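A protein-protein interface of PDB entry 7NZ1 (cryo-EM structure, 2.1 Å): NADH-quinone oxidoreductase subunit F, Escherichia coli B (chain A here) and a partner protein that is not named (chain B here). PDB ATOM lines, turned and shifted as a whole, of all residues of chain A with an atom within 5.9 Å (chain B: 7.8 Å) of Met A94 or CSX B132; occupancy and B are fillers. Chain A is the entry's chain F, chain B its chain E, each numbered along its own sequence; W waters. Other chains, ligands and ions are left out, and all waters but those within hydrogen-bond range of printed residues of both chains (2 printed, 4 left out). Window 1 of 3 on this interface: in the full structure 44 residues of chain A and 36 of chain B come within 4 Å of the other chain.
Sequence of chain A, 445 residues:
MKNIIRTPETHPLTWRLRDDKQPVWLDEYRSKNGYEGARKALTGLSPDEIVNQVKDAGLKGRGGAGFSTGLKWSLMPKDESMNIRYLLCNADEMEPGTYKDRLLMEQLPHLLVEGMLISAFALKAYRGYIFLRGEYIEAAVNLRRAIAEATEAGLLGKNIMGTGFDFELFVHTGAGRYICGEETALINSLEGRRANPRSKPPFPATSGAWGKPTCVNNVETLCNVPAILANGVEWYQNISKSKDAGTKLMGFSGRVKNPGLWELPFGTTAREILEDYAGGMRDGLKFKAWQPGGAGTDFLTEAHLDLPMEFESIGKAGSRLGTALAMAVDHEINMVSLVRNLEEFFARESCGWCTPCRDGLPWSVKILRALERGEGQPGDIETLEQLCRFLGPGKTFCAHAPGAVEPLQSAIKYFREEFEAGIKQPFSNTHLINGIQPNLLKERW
The backbone carbonyl oxygen (O) of Gly A176 is in hydrogen-bond range of the side-chain hydroxyl (OG) of Ser B77, at 2.6 Å.
The guanidinium group (NH2) of Arg A348 lies within salt-bridge range of the side-chain carboxylate (OD1) of Asp B93 (2.9 Å).
The guanidinium group (NH2) of Arg A348 lies close to N of CSX B132 (3.5 Å).
The backbone carbonyl oxygen (O) of Cys B133 lies within hydrogen-bond range of the guanidinium group (NH2) of Arg A133 (2.9 Å).
The guanidinium group (NH1) of Arg B90 is in salt-bridge range of the side-chain carboxylate (OE2) of Glu A135, 3.5 Å away.
Of the 14 printed residues of chain A, 10 touch a printed residue of chain B.
Printed residues of chain A that touch a printed residue of chain B: Met A94, Glu A95, Pro A96, Thr A98, Arg A133, Glu A135, Gly A176, Arg A177, Phe A345 and Arg A348.
Hydrophobic or aromatic side chains of chain A that line the printed part of chain B: Met A94, Pro A96 and Phe A345.
Of the 17 printed residues of chain B, 11 touch a printed residue of chain A.
Hydrophobic or aromatic side chains of chain B within 4 Å of the printed part of chain A: Val B95 and Leu B134.
Water W2 lies within hydrogen-bond range of the backbone carbonyl oxygen of Met A94 (2.5 Å) and the backbone carbonyl oxygen of Cys B133 (2.8 Å).
Water W1 lies within hydrogen-bond range of OD1 of Asp B93 (2.7 Å), NH2 of Arg A348 (3.0 Å) and OG of Ser B94 (3.2 Å).
Met A94 touches just one residue of chain B: CSX B132 (3.7 Å).
Printed residues of chain B within 4 Å of Arg A177: Ser B77 (3.8 Å).
Glu A349 touches none of the printed residues of chain B.
Of the printed residues of chain A, Gln B78 touches Glu A135 (3.8 Å).
Of the printed residues of chain A, Val B95 touches Pro A96.
Of chain A, only Met A94, Arg A133, Phe A345 and Arg A348 come within 4 Å of CSX B132.
The nearest residue of chain B that does not touch Met A94 is Cys B133 (4.7 Å).
The nearest residue of chain A that does not touch CSX B132 is Glu A349 (4.1 Å).
The nearest printed residue of chain A that does not touch Thr B131 is Glu A135 (5.6 Å).
The guanidinium group (NH1) of Arg A177 lies within hydrogen-bond range of the backbone carbonyl oxygen (O) of Arg A348 (3.2 Å).
SD of Met A94 lies within hydrogen-bond range of NH2 of Arg A133 (3.4 Å).
The side-chain hydroxyl (OG1) of Thr B131 sits close to OD of CSX B132 (3.3 Å).
O of Glu A93 sits at hydrogen-bond distance from NH1 of Arg A133 (2.8 Å).
SG of Cys B92 sits close to O of CSX B132 (3.7 Å).
The side-chain carboxylate of Glu A95 is in hydrogen-bond range of the side-chain hydroxyl of Tyr A178 (3.0 Å).
Met A94 touches CSX B132.
Cys B133 touches Glu A95 (SG to O, 3.96 Å).
Ser B94 touches Pro A96 (CB to CB, 3.9 Å).
Val B95 touches Pro A96 (CG1 to CB, 3.9 Å).
Cys B133 touches Pro A96.
C of Leu B134 touches NH1 of Arg A133 (3.5 Å).
Gly B135 touches Arg A133.
OE2 of Glu A135 touches CG of Gln B78, 3.8 Å away.
N of Ser B77 touches NE of Arg A177 (3.8 Å).
Phe A345 touches CSX B132 (CE1 to CB, 3.8 Å).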
ATOM      1  N   ASP A  92      15.966   1.942  12.762  1.00  0.00           N
ATOM      2  CA  ASP A  92      16.113   2.108  14.204  1.00  0.00           C
ATOM      3  C   ASP A  92      17.538   1.785  14.642  1.00  0.00           C
ATOM      4  O   ASP A  92      18.236   2.671  15.136  1.00  0.00           O
ATOM      5  CB  ASP A  92      15.082   1.251  14.945  1.00  0.00           C
ATOM      6  CG  ASP A  92      14.750   1.791  16.331  1.00  0.00           C
ATOM      7  OD1 ASP A  92      14.548   3.013  16.470  1.00  0.00           O
ATOM      8  OD2 ASP A  92      14.662   0.985  17.280  1.00  0.00           O
ATOM      9  N   GLU A  93      18.010   0.558  14.366  1.00  0.00           N
ATOM     10  CA  GLU A  93      19.371   0.069  14.664  1.00  0.00           C
ATOM     11  C   GLU A  93      19.759   0.331  16.130  1.00  0.00           C
ATOM     12  O   GLU A  93      20.582   1.186  16.460  1.00  0.00           O
ATOM     13  CB  GLU A  93      20.387   0.651  13.660  1.00  0.00           C
ATOM     14  CG  GLU A  93      21.858   0.177  13.776  1.00  0.00           C
ATOM     15  CD  GLU A  93      22.538  -0.128  12.469  1.00  0.00           C
ATOM     16  OE1 GLU A  93      22.192  -1.138  11.834  1.00  0.00           O
ATOM     17  OE2 GLU A  93      23.403   0.673  12.063  1.00  0.00           O
ATOM     18  N   MET A  94      19.030  -0.311  17.031  1.00  0.00           N
ATOM     19  CA  MET A  94      19.317  -0.165  18.449  1.00  0.00           C
ATOM     20  C   MET A  94      19.915  -1.410  19.088  1.00  0.00           C
ATOM     21  O   MET A  94      20.239  -1.374  20.280  1.00  0.00           O
ATOM     22  CB  MET A  94      18.052   0.252  19.201  1.00  0.00           C
ATOM     23  CG  MET A  94      17.537   1.625  18.833  1.00  0.00           C
ATOM     24  SD  MET A  94      18.330   2.896  19.822  1.00  0.00           S
ATOM     25  CE  MET A  94      17.509   2.636  21.387  1.00  0.00           C
ATOM     26  N   GLU A  95      20.092  -2.488  18.341  1.00  0.00           N
ATOM     27  CA  GLU A  95      20.688  -3.685  18.922  1.00  0.00           C
ATOM     28  C   GLU A  95      22.188  -3.472  19.094  1.00  0.00           C
ATOM     29  O   GLU A  95      22.829  -2.916  18.198  1.00  0.00           O
ATOM     30  CB  GLU A  95      20.410  -4.913  18.057  1.00  0.00           C
ATOM     31  CG  GLU A  95      21.025  -6.197  18.602  1.00  0.00           C
ATOM     32  CD  GLU A  95      20.237  -7.441  18.253  1.00  0.00           C
ATOM     33  OE1 GLU A  95      19.235  -7.716  18.945  1.00  0.00           O
ATOM     34  OE2 GLU A  95      20.626  -8.158  17.306  1.00  0.00           O
ATOM     35  N   PRO A  96      22.752  -3.812  20.255  1.00  0.00           N
ATOM     36  CA  PRO A  96      24.201  -3.669  20.451  1.00  0.00           C
ATOM     37  C   PRO A  96      24.992  -4.578  19.526  1.00  0.00           C
ATOM     38  O   PRO A  96      24.673  -5.754  19.350  1.00  0.00           O
ATOM     39  CB  PRO A  96      24.398  -4.045  21.922  1.00  0.00           C
ATOM     40  CG  PRO A  96      23.071  -3.828  22.559  1.00  0.00           C
ATOM     41  CD  PRO A  96      22.045  -4.104  21.509  1.00  0.00           C
ATOM     42  N   THR A  98      25.329  -3.662  16.328  1.00  0.00           N
ATOM     43  CA  THR A  98      24.753  -3.418  15.012  1.00  0.00           C
ATOM     44  C   THR A  98      25.090  -1.991  14.595  1.00  0.00           C
ATOM     45  O   THR A  98      24.580  -1.032  15.177  1.00  0.00           O
ATOM     46  CB  THR A  98      23.245  -3.647  15.003  1.00  0.00           C
ATOM     47  OG1 THR A  98      22.928  -4.792  15.804  1.00  0.00           O
ATOM     48  CG2 THR A  98      22.769  -3.883  13.596  1.00  0.00           C
ATOM     49  N   ARG A 133      16.663   6.635  14.104  1.00  0.00           N
ATOM     50  CA  ARG A 133      16.931   6.893  15.511  1.00  0.00           C
ATOM     51  C   ARG A 133      17.461   8.311  15.686  1.00  0.00           C
ATOM     52  O   ARG A 133      18.096   8.878  14.793  1.00  0.00           O
ATOM     53  CB  ARG A 133      17.914   5.864  16.090  1.00  0.00           C
ATOM     54  CG  ARG A 133      19.351   5.963  15.594  1.00  0.00           C
ATOM     55  CD  ARG A 133      20.259   4.912  16.227  1.00  0.00           C
ATOM     56  NE  ARG A 133      20.416   5.080  17.666  1.00  0.00           N
ATOM     57  CZ  ARG A 133      21.170   4.303  18.431  1.00  0.00           C
ATOM     58  NH1 ARG A 133      21.828   3.270  17.931  1.00  0.00           N
ATOM     59  NH2 ARG A 133      21.258   4.563  19.729  1.00  0.00           N
ATOM     60  N   GLU A 135      19.779   9.442  17.608  1.00  0.00           N
ATOM     61  CA  GLU A 135      21.199   9.568  17.895  1.00  0.00           C
ATOM     62  C   GLU A 135      21.991   9.791  16.618  1.00  0.00           C
ATOM     63  O   GLU A 135      23.075  10.386  16.654  1.00  0.00           O
ATOM     64  CB  GLU A 135      21.726   8.319  18.616  1.00  0.00           C
ATOM     65  CG  GLU A 135      21.262   8.092  20.072  1.00  0.00           C
ATOM     66  CD  GLU A 135      19.777   7.789  20.209  1.00  0.00           C
ATOM     67  OE1 GLU A 135      19.334   6.743  19.703  1.00  0.00           O
ATOM     68  OE2 GLU A 135      19.050   8.607  20.809  1.00  0.00           O
ATOM     69  N   GLY A 176      14.363   7.191  21.244  1.00  0.00           N
ATOM     70  CA  GLY A 176      15.288   6.345  21.983  1.00  0.00           C
ATOM     71  C   GLY A 176      14.793   5.156  22.789  1.00  0.00           C
ATOM     72  O   GLY A 176      15.072   5.074  23.986  1.00  0.00           O
ATOM     73  N   ARG A 177      14.050   4.240  22.172  1.00  0.00           N
ATOM     74  CA  ARG A 177      13.713   2.965  22.795  1.00  0.00           C
ATOM     75  C   ARG A 177      14.009   1.831  21.821  1.00  0.00           C
ATOM     76  O   ARG A 177      13.713   1.944  20.629  1.00  0.00           O
ATOM     77  CB  ARG A 177      12.248   2.909  23.235  1.00  0.00           C
ATOM     78  CG  ARG A 177      11.945   3.627  24.535  1.00  0.00           C
ATOM     79  CD  ARG A 177      12.460   2.890  25.749  1.00  0.00           C
ATOM     80  NE  ARG A 177      12.480   3.745  26.928  1.00  0.00           N
ATOM     81  CZ  ARG A 177      13.020   3.408  28.091  1.00  0.00           C
ATOM     82  NH1 ARG A 177      13.611   2.239  28.265  1.00  0.00           N
ATOM     83  NH2 ARG A 177      12.962   4.266  29.106  1.00  0.00           N
ATOM     84  N   TYR A 178      14.620   0.755  22.330  1.00  0.00           N
ATOM     85  CA  TYR A 178      15.046  -0.358  21.480  1.00  0.00           C
ATOM     86  C   TYR A 178      13.851  -1.121  20.909  1.00  0.00           C
ATOM     87  O   TYR A 178      13.921  -1.623  19.783  1.00  0.00           O
ATOM     88  CB  TYR A 178      15.967  -1.302  22.273  1.00  0.00           C
ATOM     89  CG  TYR A 178      16.183  -2.684  21.671  1.00  0.00           C
ATOM     90  CD1 TYR A 178      16.783  -2.841  20.419  1.00  0.00           C
ATOM     91  CD2 TYR A 178      15.791  -3.828  22.352  1.00  0.00           C
ATOM     92  CE1 TYR A 178      16.978  -4.089  19.870  1.00  0.00           C
ATOM     93  CE2 TYR A 178      15.987  -5.081  21.815  1.00  0.00           C
ATOM     94  CZ  TYR A 178      16.577  -5.206  20.571  1.00  0.00           C
ATOM     95  OH  TYR A 178      16.773  -6.451  20.027  1.00  0.00           O
ATOM     96  N   PHE A 345      20.820  -4.495  29.864  1.00  0.00           N
ATOM     97  CA  PHE A 345      20.271  -3.799  28.705  1.00  0.00           C
ATOM     98  C   PHE A 345      18.879  -4.319  28.358  1.00  0.00           C
ATOM     99  O   PHE A 345      17.947  -3.534  28.154  1.00  0.00           O
ATOM    100  CB  PHE A 345      21.220  -3.933  27.507  1.00  0.00           C
ATOM    101  CG  PHE A 345      20.582  -3.603  26.178  1.00  0.00           C
ATOM    102  CD1 PHE A 345      20.470  -2.281  25.775  1.00  0.00           C
ATOM    103  CD2 PHE A 345      20.152  -4.604  25.307  1.00  0.00           C
ATOM    104  CE1 PHE A 345      19.902  -1.960  24.561  1.00  0.00           C
ATOM    105  CE2 PHE A 345      19.568  -4.283  24.104  1.00  0.00           C
ATOM    106  CZ  PHE A 345      19.450  -2.961  23.727  1.00  0.00           C
ATOM    107  N   ARG A 348      16.063  -3.398  31.052  1.00  0.00           N
ATOM    108  CA  ARG A 348      15.667  -1.995  31.051  1.00  0.00           C
ATOM    109  C   ARG A 348      15.033  -1.554  29.732  1.00  0.00           C
ATOM    110  O   ARG A 348      14.397  -0.496  29.697  1.00  0.00           O
ATOM    111  CB  ARG A 348      16.867  -1.110  31.408  1.00  0.00           C
ATOM    112  CG  ARG A 348      17.794  -0.787  30.269  1.00  0.00           C
ATOM    113  CD  ARG A 348      19.024  -0.029  30.753  1.00  0.00           C
ATOM    114  NE  ARG A 348      19.858   0.390  29.635  1.00  0.00           N
ATOM    115  CZ  ARG A 348      20.971   1.100  29.749  1.00  0.00           C
ATOM    116  NH1 ARG A 348      21.421   1.494  30.927  1.00  0.00           N
ATOM    117  NH2 ARG A 348      21.642   1.430  28.651  1.00  0.00           N
ATOM    118  N   GLU A 349      15.200  -2.320  28.653  1.00  0.00           N
ATOM    119  CA  GLU A 349      14.576  -2.020  27.369  1.00  0.00           C
ATOM    120  C   GLU A 349      13.248  -2.740  27.149  1.00  0.00           C
ATOM    121  O   GLU A 349      12.709  -2.678  26.042  1.00  0.00           O
ATOM    122  CB  GLU A 349      15.531  -2.335  26.212  1.00  0.00           C
ATOM    123  CG  GLU A 349      16.689  -1.343  26.042  1.00  0.00           C
ATOM    124  CD  GLU A 349      16.275   0.123  25.929  1.00  0.00           C
ATOM    125  OE1 GLU A 349      15.222   0.436  25.340  1.00  0.00           O
ATOM    126  OE2 GLU A 349      17.023   0.979  26.443  1.00  0.00           O
ATOM    127  N   SER B  77      13.110   7.461  26.654  1.00  0.00           N
ATOM    128  CA  SER B  77      14.253   7.820  27.497  1.00  0.00           C
ATOM    129  C   SER B  77      14.819   9.202  27.180  1.00  0.00           C
ATOM    130  O   SER B  77      15.204   9.936  28.095  1.00  0.00           O
ATOM    131  CB  SER B  77      15.350   6.760  27.367  1.00  0.00           C
ATOM    132  OG  SER B  77      15.742   6.579  26.020  1.00  0.00           O
ATOM    133  N   GLN B  78      14.925   9.559  25.899  1.00  0.00           N
ATOM    134  CA  GLN B  78      15.559  10.828  25.540  1.00  0.00           C
ATOM    135  C   GLN B  78      14.694  12.040  25.868  1.00  0.00           C
ATOM    136  O   GLN B  78      15.237  13.123  26.113  1.00  0.00           O
ATOM    137  CB  GLN B  78      15.980  10.827  24.074  1.00  0.00           C
ATOM    138  CG  GLN B  78      16.971   9.721  23.768  1.00  0.00           C
ATOM    139  CD  GLN B  78      18.036   9.581  24.850  1.00  0.00           C
ATOM    140  OE1 GLN B  78      18.831  10.494  25.087  1.00  0.00           O
ATOM    141  NE2 GLN B  78      18.043   8.438  25.519  1.00  0.00           N
ATOM    142  N   ARG B  90      26.193  11.472  27.348  1.00  0.00           N
ATOM    143  CA  ARG B  90      25.618  10.132  27.219  1.00  0.00           C
ATOM    144  C   ARG B  90      26.679   9.130  26.771  1.00  0.00           C
ATOM    145  O   ARG B  90      27.040   9.096  25.594  1.00  0.00           O
ATOM    146  CB  ARG B  90      24.431  10.145  26.266  1.00  0.00           C
ATOM    147  CG  ARG B  90      23.152  10.602  26.929  1.00  0.00           C
ATOM    148  CD  ARG B  90      22.006  10.604  25.953  1.00  0.00           C
ATOM    149  NE  ARG B  90      22.457  10.789  24.580  1.00  0.00           N
ATOM    150  CZ  ARG B  90      21.958  10.147  23.536  1.00  0.00           C
ATOM    151  NH1 ARG B  90      21.018   9.227  23.674  1.00  0.00           N
ATOM    152  NH2 ARG B  90      22.431  10.416  22.322  1.00  0.00           N
ATOM    153  N   TYR B  91      27.171   8.315  27.701  1.00  0.00           N
ATOM    154  CA  TYR B  91      28.191   7.312  27.416  1.00  0.00           C
ATOM    155  C   TYR B  91      27.554   5.939  27.220  1.00  0.00           C
ATOM    156  O   TYR B  91      26.620   5.567  27.936  1.00  0.00           O
ATOM    157  CB  TYR B  91      29.251   7.273  28.529  1.00  0.00           C
ATOM    158  CG  TYR B  91      28.785   6.767  29.883  1.00  0.00           C
ATOM    159  CD1 TYR B  91      28.219   7.637  30.809  1.00  0.00           C
ATOM    160  CD2 TYR B  91      28.946   5.436  30.252  1.00  0.00           C
ATOM    161  CE1 TYR B  91      27.798   7.189  32.047  1.00  0.00           C
ATOM    162  CE2 TYR B  91      28.521   4.977  31.486  1.00  0.00           C
ATOM    163  CZ  TYR B  91      27.953   5.858  32.379  1.00  0.00           C
ATOM    164  OH  TYR B  91      27.536   5.404  33.607  1.00  0.00           O
ATOM    165  N   CYS B  92      28.051   5.205  26.226  1.00  0.00           N
ATOM    166  CA  CYS B  92      27.541   3.875  25.911  1.00  0.00           C
ATOM    167  C   CYS B  92      27.957   2.865  26.972  1.00  0.00           C
ATOM    168  O   CYS B  92      29.116   2.838  27.395  1.00  0.00           O
ATOM    169  CB  CYS B  92      28.048   3.426  24.541  1.00  0.00           C
ATOM    170  SG  CYS B  92      27.549   1.754  24.050  1.00  0.00           S
ATOM    171  N   ASP B  93      27.007   2.037  27.413  1.00  0.00           N
ATOM    172  CA  ASP B  93      27.310   0.979  28.366  1.00  0.00           C
ATOM    173  C   ASP B  93      26.816  -0.383  27.876  1.00  0.00           C
ATOM    174  O   ASP B  93      26.484  -1.257  28.679  1.00  0.00           O
ATOM    175  CB  ASP B  93      26.756   1.318  29.759  1.00  0.00           C
ATOM    176  CG  ASP B  93      25.225   1.316  29.850  1.00  0.00           C
ATOM    177  OD1 ASP B  93      24.518   1.377  28.833  1.00  0.00           O
ATOM    178  OD2 ASP B  93      24.725   1.259  30.990  1.00  0.00           O
ATOM    179  N   SER B  94      26.794  -0.593  26.565  1.00  0.00           N
ATOM    180  CA  SER B  94      26.310  -1.851  26.020  1.00  0.00           C
ATOM    181  C   SER B  94      27.473  -2.836  25.934  1.00  0.00           C
ATOM    182  O   SER B  94      28.550  -2.594  26.477  1.00  0.00           O
ATOM    183  CB  SER B  94      25.619  -1.633  24.678  1.00  0.00           C
ATOM    184  OG  SER B  94      24.633  -0.632  24.783  1.00  0.00           O
ATOM    185  N   VAL B  95      27.284  -3.935  25.204  1.00  0.00           N
ATOM    186  CA  VAL B  95      28.185  -5.079  25.324  1.00  0.00           C
ATOM    187  C   VAL B  95      29.514  -4.867  24.584  1.00  0.00           C
ATOM    188  O   VAL B  95      30.571  -5.252  25.095  1.00  0.00           O
ATOM    189  CB  VAL B  95      27.444  -6.375  24.908  1.00  0.00           C
ATOM    190  CG1 VAL B  95      27.052  -6.422  23.431  1.00  0.00           C
ATOM    191  CG2 VAL B  95      28.250  -7.600  25.277  1.00  0.00           C
ATOM    192  N   CYS B  97      30.948  -1.978  23.883  1.00  0.00           N
ATOM    193  CA  CYS B  97      31.681  -0.933  24.573  1.00  0.00           C
ATOM    194  C   CYS B  97      32.177  -1.422  25.931  1.00  0.00           C
ATOM    195  O   CYS B  97      33.163  -0.893  26.449  1.00  0.00           O
ATOM    196  CB  CYS B  97      30.801   0.309  24.704  1.00  0.00           C
ATOM    197  SG  CYS B  97      30.884   1.410  23.259  1.00  0.00           S
ATOM    198  N   LEU B 129      24.688  10.685  32.110  1.00  0.00           N
ATOM    199  CA  LEU B 129      23.681   9.652  31.888  1.00  0.00           C
ATOM    200  C   LEU B 129      24.253   8.468  31.113  1.00  0.00           C
ATOM    201  O   LEU B 129      24.939   8.672  30.102  1.00  0.00           O
ATOM    202  CB  LEU B 129      22.484  10.236  31.131  1.00  0.00           C
ATOM    203  CG  LEU B 129      21.349  10.792  31.989  1.00  0.00           C
ATOM    204  CD1 LEU B 129      20.340  11.536  31.130  1.00  0.00           C
ATOM    205  CD2 LEU B 129      20.682   9.681  32.771  1.00  0.00           C
ATOM    206  N   PRO B 130      24.004   7.236  31.545  1.00  0.00           N
ATOM    207  CA  PRO B 130      24.319   6.090  30.688  1.00  0.00           C
ATOM    208  C   PRO B 130      23.322   5.986  29.544  1.00  0.00           C
ATOM    209  O   PRO B 130      22.184   6.450  29.637  1.00  0.00           O
ATOM    210  CB  PRO B 130      24.200   4.895  31.635  1.00  0.00           C
ATOM    211  CG  PRO B 130      23.197   5.331  32.630  1.00  0.00           C
ATOM    212  CD  PRO B 130      23.356   6.819  32.800  1.00  0.00           C
ATOM    213  N   THR B 131      23.760   5.373  28.456  1.00  0.00           N
ATOM    214  CA  THR B 131      22.865   5.153  27.329  1.00  0.00           C
ATOM    215  C   THR B 131      23.163   3.838  26.633  1.00  0.00           C
ATOM    216  O   THR B 131      24.247   3.289  26.778  1.00  0.00           O
ATOM    217  CB  THR B 131      22.942   6.312  26.302  1.00  0.00           C
ATOM    218  OG1 THR B 131      21.922   6.148  25.313  1.00  0.00           O
ATOM    219  CG2 THR B 131      24.311   6.381  25.621  1.00  0.00           C
ATOM    220  N   CSX B 132      22.213   3.356  25.838  1.00  0.00           N
ATOM    221  CA  CSX B 132      22.391   2.137  25.082  1.00  0.00           C
ATOM    222  CB  CSX B 132      21.066   1.656  24.504  1.00  0.00           C
ATOM    223  SG  CSX B 132      19.853   2.901  24.248  1.00  0.00           S
ATOM    224  C   CSX B 132      23.411   2.285  23.949  1.00  0.00           C
ATOM    225  O   CSX B 132      24.141   3.276  23.833  1.00  0.00           O
ATOM    226  OD  CSX B 132      20.465   3.907  23.324  1.00  0.00           O
ATOM    227  N   CYS B 133      23.474   1.267  23.095  1.00  0.00           N
ATOM    228  CA  CYS B 133      24.491   1.240  22.048  1.00  0.00           C
ATOM    229  C   CYS B 133      24.208   2.297  20.993  1.00  0.00           C
ATOM    230  O   CYS B 133      23.103   2.401  20.474  1.00  0.00           O
ATOM    231  CB  CYS B 133      24.581  -0.137  21.405  1.00  0.00           C
ATOM    232  SG  CYS B 133      25.199  -0.133  19.709  1.00  0.00           S
ATOM    233  N   LEU B 134      25.234   3.084  20.708  1.00  0.00           N
ATOM    234  CA  LEU B 134      25.119   4.243  19.842  1.00  0.00           C
ATOM    235  C   LEU B 134      25.264   3.899  18.371  1.00  0.00           C
ATOM    236  O   LEU B 134      25.200   4.803  17.534  1.00  0.00           O
ATOM    237  CB  LEU B 134      26.162   5.292  20.237  1.00  0.00           C
ATOM    238  CG  LEU B 134      25.904   6.013  21.559  1.00  0.00           C
ATOM    239  CD1 LEU B 134      27.175   6.633  22.080  1.00  0.00           C
ATOM    240  CD2 LEU B 134      24.825   7.066  21.386  1.00  0.00           C
ATOM    241  N   GLY B 135      25.505   2.635  18.034  1.00  0.00           N
ATOM    242  CA  GLY B 135      25.653   2.290  16.642  1.00  0.00           C
ATOM    243  C   GLY B 135      27.033   2.552  16.100  1.00  0.00           C
ATOM    244  O   GLY B 135      27.194   2.645  14.883  1.00  0.00           O
ATOM    245  N   ASN B 142      32.350   4.788  23.150  1.00  0.00           N
ATOM    246  CA  ASN B 142      31.648   5.901  22.530  1.00  0.00           C
ATOM    247  C   ASN B 142      30.915   6.717  23.582  1.00  0.00           C
ATOM    248  O   ASN B 142      30.459   6.185  24.597  1.00  0.00           O
ATOM    249  CB  ASN B 142      30.644   5.396  21.495  1.00  0.00           C
ATOM    250  CG  ASN B 142      31.298   4.988  20.197  1.00  0.00           C
ATOM    251  OD1 ASN B 142      31.840   5.820  19.476  1.00  0.00           O
ATOM    252  ND2 ASN B 142      31.286   3.695  19.913  1.00  0.00           N
HETATM  253  O   HOH W   1      23.417  -0.783  27.714  1.00  0.00           O
HETATM  254  O   HOH W   2      20.917   0.865  21.281  1.00  0.00           O
